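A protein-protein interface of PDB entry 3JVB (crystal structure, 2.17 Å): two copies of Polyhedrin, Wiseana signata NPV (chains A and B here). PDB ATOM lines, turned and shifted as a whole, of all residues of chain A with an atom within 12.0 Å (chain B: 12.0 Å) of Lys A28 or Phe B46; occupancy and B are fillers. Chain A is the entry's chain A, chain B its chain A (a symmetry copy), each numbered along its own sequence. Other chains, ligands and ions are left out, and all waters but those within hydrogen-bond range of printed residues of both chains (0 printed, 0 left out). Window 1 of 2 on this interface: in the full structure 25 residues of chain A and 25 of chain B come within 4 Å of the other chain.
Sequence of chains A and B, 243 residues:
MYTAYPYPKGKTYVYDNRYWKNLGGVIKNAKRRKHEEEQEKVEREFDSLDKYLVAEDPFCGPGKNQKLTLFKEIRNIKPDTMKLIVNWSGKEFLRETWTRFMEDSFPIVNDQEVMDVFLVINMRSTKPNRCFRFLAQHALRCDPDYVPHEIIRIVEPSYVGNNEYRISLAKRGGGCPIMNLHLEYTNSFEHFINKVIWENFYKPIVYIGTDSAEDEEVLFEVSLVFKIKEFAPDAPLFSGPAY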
ATOM      1  N   GLY A  10      33.357  17.901  13.821  1.00  0.00           N
ATOM      2  CA  GLY A  10      32.298  18.898  13.945  1.00  0.00           C
ATOM      3  C   GLY A  10      31.744  18.923  15.351  1.00  0.00           C
ATOM      4  O   GLY A  10      31.491  17.869  15.919  1.00  0.00           O
ATOM      5  N   LYS A  11      31.581  20.108  15.940  1.00  0.00           N
ATOM      6  CA  LYS A  11      31.122  20.226  17.325  1.00  0.00           C
ATOM      7  C   LYS A  11      29.670  20.684  17.479  1.00  0.00           C
ATOM      8  O   LYS A  11      28.943  20.813  16.490  1.00  0.00           O
ATOM      9  CB  LYS A  11      32.092  21.128  18.125  1.00  0.00           C
ATOM     10  N   LYS A  21      25.351  23.326  14.784  1.00  0.00           N
ATOM     11  CA  LYS A  21      26.274  22.291  14.301  1.00  0.00           C
ATOM     12  C   LYS A  21      27.007  22.792  13.087  1.00  0.00           C
ATOM     13  O   LYS A  21      26.465  23.612  12.346  1.00  0.00           O
ATOM     14  CB  LYS A  21      25.526  20.982  13.947  1.00  0.00           C
ATOM     15  CG  LYS A  21      24.819  20.323  15.127  1.00  0.00           C
ATOM     16  CD  LYS A  21      25.512  19.046  15.561  1.00  0.00           C
ATOM     17  CE  LYS A  21      24.903  18.458  16.809  1.00  0.00           C
ATOM     18  NZ  LYS A  21      23.554  17.866  16.582  1.00  0.00           N
ATOM     19  N   ASN A  22      28.224  22.270  12.862  1.00  0.00           N
ATOM     20  CA  ASN A  22      29.058  22.613  11.717  1.00  0.00           C
ATOM     21  C   ASN A  22      28.414  22.152  10.420  1.00  0.00           C
ATOM     22  O   ASN A  22      27.903  21.033  10.332  1.00  0.00           O
ATOM     23  CB  ASN A  22      30.485  22.088  11.888  1.00  0.00           C
ATOM     24  CG  ASN A  22      31.188  22.692  13.086  1.00  0.00           C
ATOM     25  OD1 ASN A  22      31.037  22.236  14.228  1.00  0.00           O
ATOM     26  ND2 ASN A  22      31.948  23.755  12.863  1.00  0.00           N
ATOM     27  N   LEU A  23      28.397  23.057   9.431  1.00  0.00           N
ATOM     28  CA  LEU A  23      27.783  22.859   8.128  1.00  0.00           C
ATOM     29  C   LEU A  23      28.290  21.641   7.350  1.00  0.00           C
ATOM     30  O   LEU A  23      27.486  20.963   6.700  1.00  0.00           O
ATOM     31  CB  LEU A  23      27.838  24.152   7.296  1.00  0.00           C
ATOM     32  CG  LEU A  23      27.140  24.150   5.926  1.00  0.00           C
ATOM     33  CD1 LEU A  23      25.676  23.746   6.033  1.00  0.00           C
ATOM     34  CD2 LEU A  23      27.319  25.472   5.225  1.00  0.00           C
ATOM     35  N   GLY A  24      29.594  21.378   7.433  1.00  0.00           N
ATOM     36  CA  GLY A  24      30.231  20.254   6.753  1.00  0.00           C
ATOM     37  C   GLY A  24      29.701  18.925   7.232  1.00  0.00           C
ATOM     38  O   GLY A  24      29.268  18.107   6.417  1.00  0.00           O
ATOM     39  N   GLY A  25      29.691  18.745   8.555  1.00  0.00           N
ATOM     40  CA  GLY A  25      29.177  17.547   9.218  1.00  0.00           C
ATOM     41  C   GLY A  25      27.721  17.281   8.888  1.00  0.00           C
ATOM     42  O   GLY A  25      27.323  16.130   8.693  1.00  0.00           O
ATOM     43  N   VAL A  26      26.929  18.359   8.791  1.00  0.00           N
ATOM     44  CA  VAL A  26      25.508  18.328   8.449  1.00  0.00           C
ATOM     45  C   VAL A  26      25.296  17.838   7.004  1.00  0.00           C
ATOM     46  O   VAL A  26      24.459  16.963   6.776  1.00  0.00           O
ATOM     47  CB  VAL A  26      24.825  19.691   8.769  1.00  0.00           C
ATOM     48  CG1 VAL A  26      23.459  19.809   8.112  1.00  0.00           C
ATOM     49  CG2 VAL A  26      24.708  19.892  10.282  1.00  0.00           C
ATOM     50  N   ILE A  27      26.081  18.367   6.053  1.00  0.00           N
ATOM     51  CA  ILE A  27      26.017  17.970   4.643  1.00  0.00           C
ATOM     52  C   ILE A  27      26.536  16.528   4.461  1.00  0.00           C
ATOM     53  O   ILE A  27      25.945  15.756   3.701  1.00  0.00           O
ATOM     54  CB  ILE A  27      26.688  19.022   3.711  1.00  0.00           C
ATOM     55  CG1 ILE A  27      25.819  20.304   3.656  1.00  0.00           C
ATOM     56  CG2 ILE A  27      26.921  18.460   2.298  1.00  0.00           C
ATOM     57  CD1 ILE A  27      26.495  21.540   3.101  1.00  0.00           C
ATOM     58  N   LYS A  28      27.589  16.159   5.217  1.00  0.00           N
ATOM     59  CA  LYS A  28      28.180  14.819   5.200  1.00  0.00           C
ATOM     60  C   LYS A  28      27.171  13.759   5.668  1.00  0.00           C
ATOM     61  O   LYS A  28      27.017  12.743   4.988  1.00  0.00           O
ATOM     62  CB  LYS A  28      29.469  14.773   6.037  1.00  0.00           C
ATOM     63  N   ASN A  29      26.450  14.020   6.785  1.00  0.00           N
ATOM     64  CA  ASN A  29      25.436  13.106   7.326  1.00  0.00           C
ATOM     65  C   ASN A  29      24.264  12.920   6.371  1.00  0.00           C
ATOM     66  O   ASN A  29      23.791  11.798   6.208  1.00  0.00           O
ATOM     67  CB  ASN A  29      24.946  13.557   8.700  1.00  0.00           C
ATOM     68  CG  ASN A  29      25.960  13.440   9.818  1.00  0.00           C
ATOM     69  OD1 ASN A  29      27.128  13.072   9.622  1.00  0.00           O
ATOM     70  ND2 ASN A  29      25.534  13.779  11.027  1.00  0.00           N
ATOM     71  N   ALA A  30      23.824  14.009   5.703  1.00  0.00           N
ATOM     72  CA  ALA A  30      22.718  13.960   4.741  1.00  0.00           C
ATOM     73  C   ALA A  30      23.107  13.208   3.466  1.00  0.00           C
ATOM     74  O   ALA A  30      22.284  12.466   2.924  1.00  0.00           O
ATOM     75  CB  ALA A  30      22.246  15.355   4.411  1.00  0.00           C
ATOM     76  N   LYS A  31      24.354  13.385   2.996  1.00  0.00           N
ATOM     77  CA  LYS A  31      24.863  12.685   1.817  1.00  0.00           C
ATOM     78  C   LYS A  31      25.112  11.206   2.134  1.00  0.00           C
ATOM     79  O   LYS A  31      25.002  10.374   1.235  1.00  0.00           O
ATOM     80  CB  LYS A  31      26.116  13.373   1.243  1.00  0.00           C
ATOM     81  CG  LYS A  31      25.782  14.638   0.462  1.00  0.00           C
ATOM     82  CD  LYS A  31      26.974  15.216  -0.285  1.00  0.00           C
ATOM     83  CE  LYS A  31      26.658  15.515  -1.737  1.00  0.00           C
ATOM     84  NZ  LYS A  31      25.653  16.604  -1.902  1.00  0.00           N
ATOM     85  N   ARG A  32      25.400  10.879   3.422  1.00  0.00           N
ATOM     86  CA  ARG A  32      25.612   9.507   3.902  1.00  0.00           C
ATOM     87  C   ARG A  32      24.302   8.721   3.870  1.00  0.00           C
ATOM     88  O   ARG A  32      24.334   7.500   3.745  1.00  0.00           O
ATOM     89  CB  ARG A  32      26.210   9.489   5.317  1.00  0.00           C
ATOM     90  N   ARG A  33      23.156   9.420   3.989  1.00  0.00           N
ATOM     91  CA  ARG A  33      21.831   8.810   3.912  1.00  0.00           C
ATOM     92  C   ARG A  33      21.477   8.559   2.442  1.00  0.00           C
ATOM     93  O   ARG A  33      20.881   7.528   2.132  1.00  0.00           O
ATOM     94  CB  ARG A  33      20.771   9.691   4.592  1.00  0.00           C
ATOM     95  N   LYS A  34      21.864   9.488   1.539  1.00  0.00           N
ATOM     96  CA  LYS A  34      21.624   9.375   0.098  1.00  0.00           C
ATOM     97  C   LYS A  34      22.469   8.264  -0.536  1.00  0.00           C
ATOM     98  O   LYS A  34      21.983   7.578  -1.434  1.00  0.00           O
ATOM     99  CB  LYS A  34      21.891  10.712  -0.612  1.00  0.00           C
ATOM    100  N   HIS A  35      23.728   8.097  -0.075  1.00  0.00           N
ATOM    101  CA  HIS A  35      24.673   7.095  -0.577  1.00  0.00           C
ATOM    102  C   HIS A  35      24.362   5.679  -0.088  1.00  0.00           C
ATOM    103  O   HIS A  35      24.437   4.738  -0.881  1.00  0.00           O
ATOM    104  CB  HIS A  35      26.121   7.488  -0.248  1.00  0.00           C
ATOM    105  N   GLU A  36      24.007   5.521   1.204  1.00  0.00           N
ATOM    106  CA  GLU A  36      23.671   4.217   1.782  1.00  0.00           C
ATOM    107  C   GLU A  36      22.252   3.769   1.410  1.00  0.00           C
ATOM    108  O   GLU A  36      21.547   4.443   0.657  1.00  0.00           O
ATOM    109  CB  GLU A  36      23.852   4.225   3.305  1.00  0.00           C
ATOM    110  N   HIS B  35      37.046   4.136  -2.743  1.00  0.00           N
ATOM    111  CA  HIS B  35      36.075   5.196  -2.457  1.00  0.00           C
ATOM    112  C   HIS B  35      36.570   6.197  -1.410  1.00  0.00           C
ATOM    113  O   HIS B  35      36.378   7.401  -1.591  1.00  0.00           O
ATOM    114  CB  HIS B  35      34.714   4.606  -2.058  1.00  0.00           C
ATOM    115  N   GLU B  36      37.210   5.711  -0.326  1.00  0.00           N
ATOM    116  CA  GLU B  36      37.742   6.573   0.734  1.00  0.00           C
ATOM    117  C   GLU B  36      39.068   7.229   0.332  1.00  0.00           C
ATOM    118  O   GLU B  36      39.548   7.063  -0.790  1.00  0.00           O
ATOM    119  CB  GLU B  36      37.901   5.797   2.047  1.00  0.00           C
ATOM    120  N   GLU B  40      38.806  11.513   0.560  1.00  0.00           N
ATOM    121  CA  GLU B  40      39.473  12.646   1.193  1.00  0.00           C
ATOM    122  C   GLU B  40      39.194  13.961   0.459  1.00  0.00           C
ATOM    123  O   GLU B  40      39.303  15.026   1.069  1.00  0.00           O
ATOM    124  CB  GLU B  40      40.983  12.391   1.314  1.00  0.00           C
ATOM    125  N   LYS B  41      38.835  13.884  -0.842  1.00  0.00           N
ATOM    126  CA  LYS B  41      38.496  15.028  -1.697  1.00  0.00           C
ATOM    127  C   LYS B  41      37.193  15.679  -1.224  1.00  0.00           C
ATOM    128  O   LYS B  41      37.080  16.910  -1.236  1.00  0.00           O
ATOM    129  CB  LYS B  41      38.362  14.586  -3.162  1.00  0.00           C
ATOM    130  N   VAL B  42      36.213  14.847  -0.809  1.00  0.00           N
ATOM    131  CA  VAL B  42      34.928  15.299  -0.278  1.00  0.00           C
ATOM    132  C   VAL B  42      35.141  15.870   1.121  1.00  0.00           C
ATOM    133  O   VAL B  42      34.486  16.846   1.479  1.00  0.00           O
ATOM    134  CB  VAL B  42      33.870  14.177  -0.276  1.00  0.00           C
ATOM    135  N   GLU B  43      36.086  15.277   1.891  1.00  0.00           N
ATOM    136  CA  GLU B  43      36.457  15.713   3.241  1.00  0.00           C
ATOM    137  C   GLU B  43      37.052  17.126   3.231  1.00  0.00           C
ATOM    138  O   GLU B  43      36.870  17.855   4.202  1.00  0.00           O
ATOM    139  CB  GLU B  43      37.430  14.721   3.895  1.00  0.00           C
ATOM    140  N   ARG B  44      37.743  17.510   2.132  1.00  0.00           N
ATOM    141  CA  ARG B  44      38.335  18.842   1.947  1.00  0.00           C
ATOM    142  C   ARG B  44      37.220  19.887   1.816  1.00  0.00           C
ATOM    143  O   ARG B  44      37.332  20.992   2.364  1.00  0.00           O
ATOM    144  CB  ARG B  44      39.227  18.869   0.695  1.00  0.00           C
ATOM    145  N   GLU B  45      36.142  19.517   1.092  1.00  0.00           N
ATOM    146  CA  GLU B  45      34.959  20.344   0.876  1.00  0.00           C
ATOM    147  C   GLU B  45      34.210  20.500   2.192  1.00  0.00           C
ATOM    148  O   GLU B  45      33.830  21.617   2.537  1.00  0.00           O
ATOM    149  CB  GLU B  45      34.051  19.726  -0.202  1.00  0.00           C
ATOM    150  N   PHE B  46      34.038  19.390   2.946  1.00  0.00           N
ATOM    151  CA  PHE B  46      33.369  19.393   4.244  1.00  0.00           C
ATOM    152  C   PHE B  46      34.150  20.170   5.306  1.00  0.00           C
ATOM    153  O   PHE B  46      33.532  20.853   6.127  1.00  0.00           O
ATOM    154  CB  PHE B  46      33.050  17.965   4.714  1.00  0.00           C
ATOM    155  CG  PHE B  46      32.134  17.170   3.812  1.00  0.00           C
ATOM    156  CD1 PHE B  46      30.955  17.723   3.324  1.00  0.00           C
ATOM    157  CD2 PHE B  46      32.416  15.844   3.505  1.00  0.00           C
ATOM    158  CE1 PHE B  46      30.108  16.985   2.496  1.00  0.00           C
ATOM    159  CE2 PHE B  46      31.565  15.105   2.677  1.00  0.00           C
ATOM    160  CZ  PHE B  46      30.412  15.680   2.185  1.00  0.00           C
ATOM    161  N   ASP B  47      35.500  20.101   5.259  1.00  0.00           N
ATOM    162  CA  ASP B  47      36.400  20.811   6.182  1.00  0.00           C
ATOM    163  C   ASP B  47      36.284  22.325   6.034  1.00  0.00           C
ATOM    164  O   ASP B  47      36.386  23.038   7.026  1.00  0.00           O
ATOM    165  CB  ASP B  47      37.859  20.368   5.990  1.00  0.00           C
ATOM    166  N   SER B  48      36.076  22.814   4.800  1.00  0.00           N
ATOM    167  CA  SER B  48      35.877  24.237   4.521  1.00  0.00           C
ATOM    168  C   SER B  48      34.460  24.651   4.935  1.00  0.00           C
ATOM    169  O   SER B  48      34.274  25.741   5.466  1.00  0.00           O
ATOM    170  CB  SER B  48      36.137  24.558   3.053  1.00  0.00           C
ATOM    171  OG  SER B  48      35.732  23.503   2.198  1.00  0.00           O
ATOM    172  N   LEU B  49      33.475  23.760   4.742  1.00  0.00           N
ATOM    173  CA  LEU B  49      32.087  24.004   5.149  1.00  0.00           C
ATOM    174  C   LEU B  49      31.962  24.025   6.681  1.00  0.00           C
ATOM    175  O   LEU B  49      31.089  24.712   7.204  1.00  0.00           O
ATOM    176  CB  LEU B  49      31.139  22.961   4.543  1.00  0.00           C
ATOM    177  CG  LEU B  49      30.851  23.076   3.050  1.00  0.00           C
ATOM    178  CD1 LEU B  49      30.183  21.822   2.530  1.00  0.00           C
ATOM    179  CD2 LEU B  49      30.013  24.297   2.730  1.00  0.00           C
ATOM    180  N   ASP B  50      32.891  23.329   7.391  1.00  0.00           N
ATOM    181  CA  ASP B  50      32.958  23.254   8.854  1.00  0.00           C
ATOM    182  C   ASP B  50      33.401  24.555   9.513  1.00  0.00           C
ATOM    183  O   ASP B  50      33.303  24.669  10.736  1.00  0.00           O
ATOM    184  CB  ASP B  50      33.823  22.071   9.321  1.00  0.00           C
ATOM    185  CG  ASP B  50      33.147  20.715   9.243  1.00  0.00           C
ATOM    186  OD1 ASP B  50      31.904  20.666   9.318  1.00  0.00           O
ATOM    187  OD2 ASP B  50      33.867  19.699   9.130  1.00  0.00           O
ATOM    188  N   LYS B  51      33.836  25.560   8.720  1.00  0.00           N
ATOM    189  CA  LYS B  51      34.180  26.876   9.272  1.00  0.00           C
ATOM    190  C   LYS B  51      32.880  27.654   9.585  1.00  0.00           C
ATOM    191  O   LYS B  51      32.921  28.721  10.199  1.00  0.00           O
ATOM    192  CB  LYS B  51      35.079  27.665   8.303  1.00  0.00           C
ATOM    193  N   TYR B  52      31.729  27.094   9.179  1.00  0.00           N
ATOM    194  CA  TYR B  52      30.416  27.712   9.347  1.00  0.00           C
ATOM    195  C   TYR B  52      29.429  26.819  10.077  1.00  0.00           C
ATOM    196  O   TYR B  52      29.567  25.594  10.061  1.00  0.00           O
ATOM    197  CB  TYR B  52      29.841  28.163   7.988  1.00  0.00           C
ATOM    198  CG  TYR B  52      30.797  29.021   7.191  1.00  0.00           C
ATOM    199  CD1 TYR B  52      30.823  30.405   7.351  1.00  0.00           C
ATOM    200  CD2 TYR B  52      31.705  28.449   6.303  1.00  0.00           C
ATOM    201  CE1 TYR B  52      31.730  31.195   6.647  1.00  0.00           C
ATOM    202  CE2 TYR B  52      32.593  29.231   5.571  1.00  0.00           C
ATOM    203  CZ  TYR B  52      32.611  30.602   5.755  1.00  0.00           C
ATOM    204  OH  TYR B  52      33.497  31.364   5.035  1.00  0.00           O
ATOM    205  N   LEU B  53      28.407  27.442  10.690  1.00  0.00           N
ATOM    206  CA  LEU B  53      27.395  26.748  11.477  1.00  0.00           C
ATOM    207  C   LEU B  53      25.974  26.955  11.004  1.00  0.00           C
ATOM    208  O   LEU B  53      25.652  28.014  10.474  1.00  0.00           O
ATOM    209  CB  LEU B  53      27.464  27.219  12.946  1.00  0.00           C
ATOM    210  CG  LEU B  53      28.787  27.171  13.670  1.00  0.00           C
ATOM    211  CD1 LEU B  53      28.673  27.888  14.987  1.00  0.00           C
ATOM    212  CD2 LEU B  53      29.244  25.736  13.892  1.00  0.00           C
ATOM    213  N   VAL B  54      25.107  25.961  11.287  1.00  0.00           N
ATOM    214  CA  VAL B  54      23.661  25.983  11.044  1.00  0.00           C
ATOM    215  C   VAL B  54      22.912  25.753  12.372  1.00  0.00           C
ATOM    216  O   VAL B  54      23.386  25.006  13.228  1.00  0.00           O
ATOM    217  CB  VAL B  54      23.158  25.028   9.910  1.00  0.00           C
ATOM    218  CG1 VAL B  54      23.558  25.531   8.531  1.00  0.00           C
ATOM    219  CG2 VAL B  54      23.587  23.586  10.130  1.00  0.00           C
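O of Asp B50 sits at hydrogen-bond distance from ND2 of Asn A22 (2.7 Å). N of Gly A24 sits at hydrogen-bond distance from OD1 of Asp B50 (3.1 Å). The backbone NH (N) of Gly A25 lies within hydrogen-bond range of the side-chain carboxylate (OD1) of Asp B50, at 3.0 Å. The backbone NH of Leu A23 is in hydrogen-bond range of the backbone carbonyl oxygen of Tyr B52. The backbone NH (N) of Val B54 is in hydrogen-bond range of the backbone carbonyl oxygen (O) of Lys A21 (2.9 Å).
The side-chain amide oxygen (OD1) of Asn A22 sits at hydrogen-bond distance from the backbone NH (N) of Lys A11, 2.8 Å away. O of Gly A25 sits close to OD1 of Asn A29, 3.2 Å away.
Among the printed residues, pairs that only touch across the chains: Leu A23 with Leu B49, Lys A21 with Leu B53, Gly A24 with Phe B46, Asn A22 with Tyr B52, Asn A22 with Leu B53, Ile A27 with Phe B46, Gly A24 with Leu B49, Leu A23 with Val B54, Ile A27 with Leu B49, Lys A28 with Phe B46 and Val A26 with Val B54.
Of chain B, only Phe B46 comes within 4 Å of Lys A28. Of chain B, only Phe B46, Leu B49 and Asp B50 come within 4 Å of Gly A24. Gly A25 touches just one residue of chain B: Asp B50 (3.0 Å). Val A26 touches one residue of chain B. Of the printed residues of chain B, Ile A27 touches Phe B46 (3.5 Å) and Leu B49 (3.7 Å). No residue of chain B comes within 4 Å of Asn A29. No residue of chain B comes within 4 Å of Ala A30. No residue of chain A comes within 4 Å of Val B42. No residue of chain A comes within 4 Å of Glu B43. No residue of chain A comes within 4 Å of Arg B44. No residue of chain A comes within 4 Å of Asp B47. Ser B48 touches none of the printed residues of chain A. Leu B49 touches three residues of chain A. Of the printed residues of chain A, Asp B50 touches Asn A22 (2.7 Å), Gly A24 (3.1 Å) and Gly A25 (3.0 Å). Of the printed residues of chain B, Lys A21 touches Leu B53 (3.4 Å) and Val B54 (2.9 Å). Of the printed residues of chain A, Leu B53 touches Lys A21 and Asn A22. Of the printed residues of chain A, Val B54 touches Lys A21, Leu A23 and Val A26. Printed residues of chain B within 4 Å of Asn A22: Asp B50 (2.7 Å), Tyr B52 (3.4 Å) and Leu B53 (3.5 Å). Of the printed residues of chain A, Tyr B52 touches Asn A22 and Leu A23. His A35 touches none of the printed residues of chain B. Lys B51 touches none of the printed residues of chain A. The nearest residue of chain A that does not touch Phe B46 is Lys A31 (4.3 Å). The nearest printed residue of chain A that does not touch Val B54 is Asn A22 (5.0 Å).
Printed residues of chain B that touch a printed residue of chain A: Phe B46, Leu B49, Asp B50, Tyr B52, Leu B53 and Val B54. Hydrophobic or aromatic side chains of chain B within 4 Å of the printed part of chain A: Phe B46, Leu B49, Leu B53 and Val B54. Along chain B the printed residues that touch a printed residue of chain A span positions 46 to 54. Among the printed residues, 16 pairs touch across the chains. Among the printed residues, no Asp or Glu carboxylate lies within 4 Å of a Lys or Arg side-chain nitrogen of the other chain.
Positions printed for both chains: 35 and 36. Of the 16 pairs that touch across the chains among the printed residues, none has its exchanged pair printed and touching as well.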
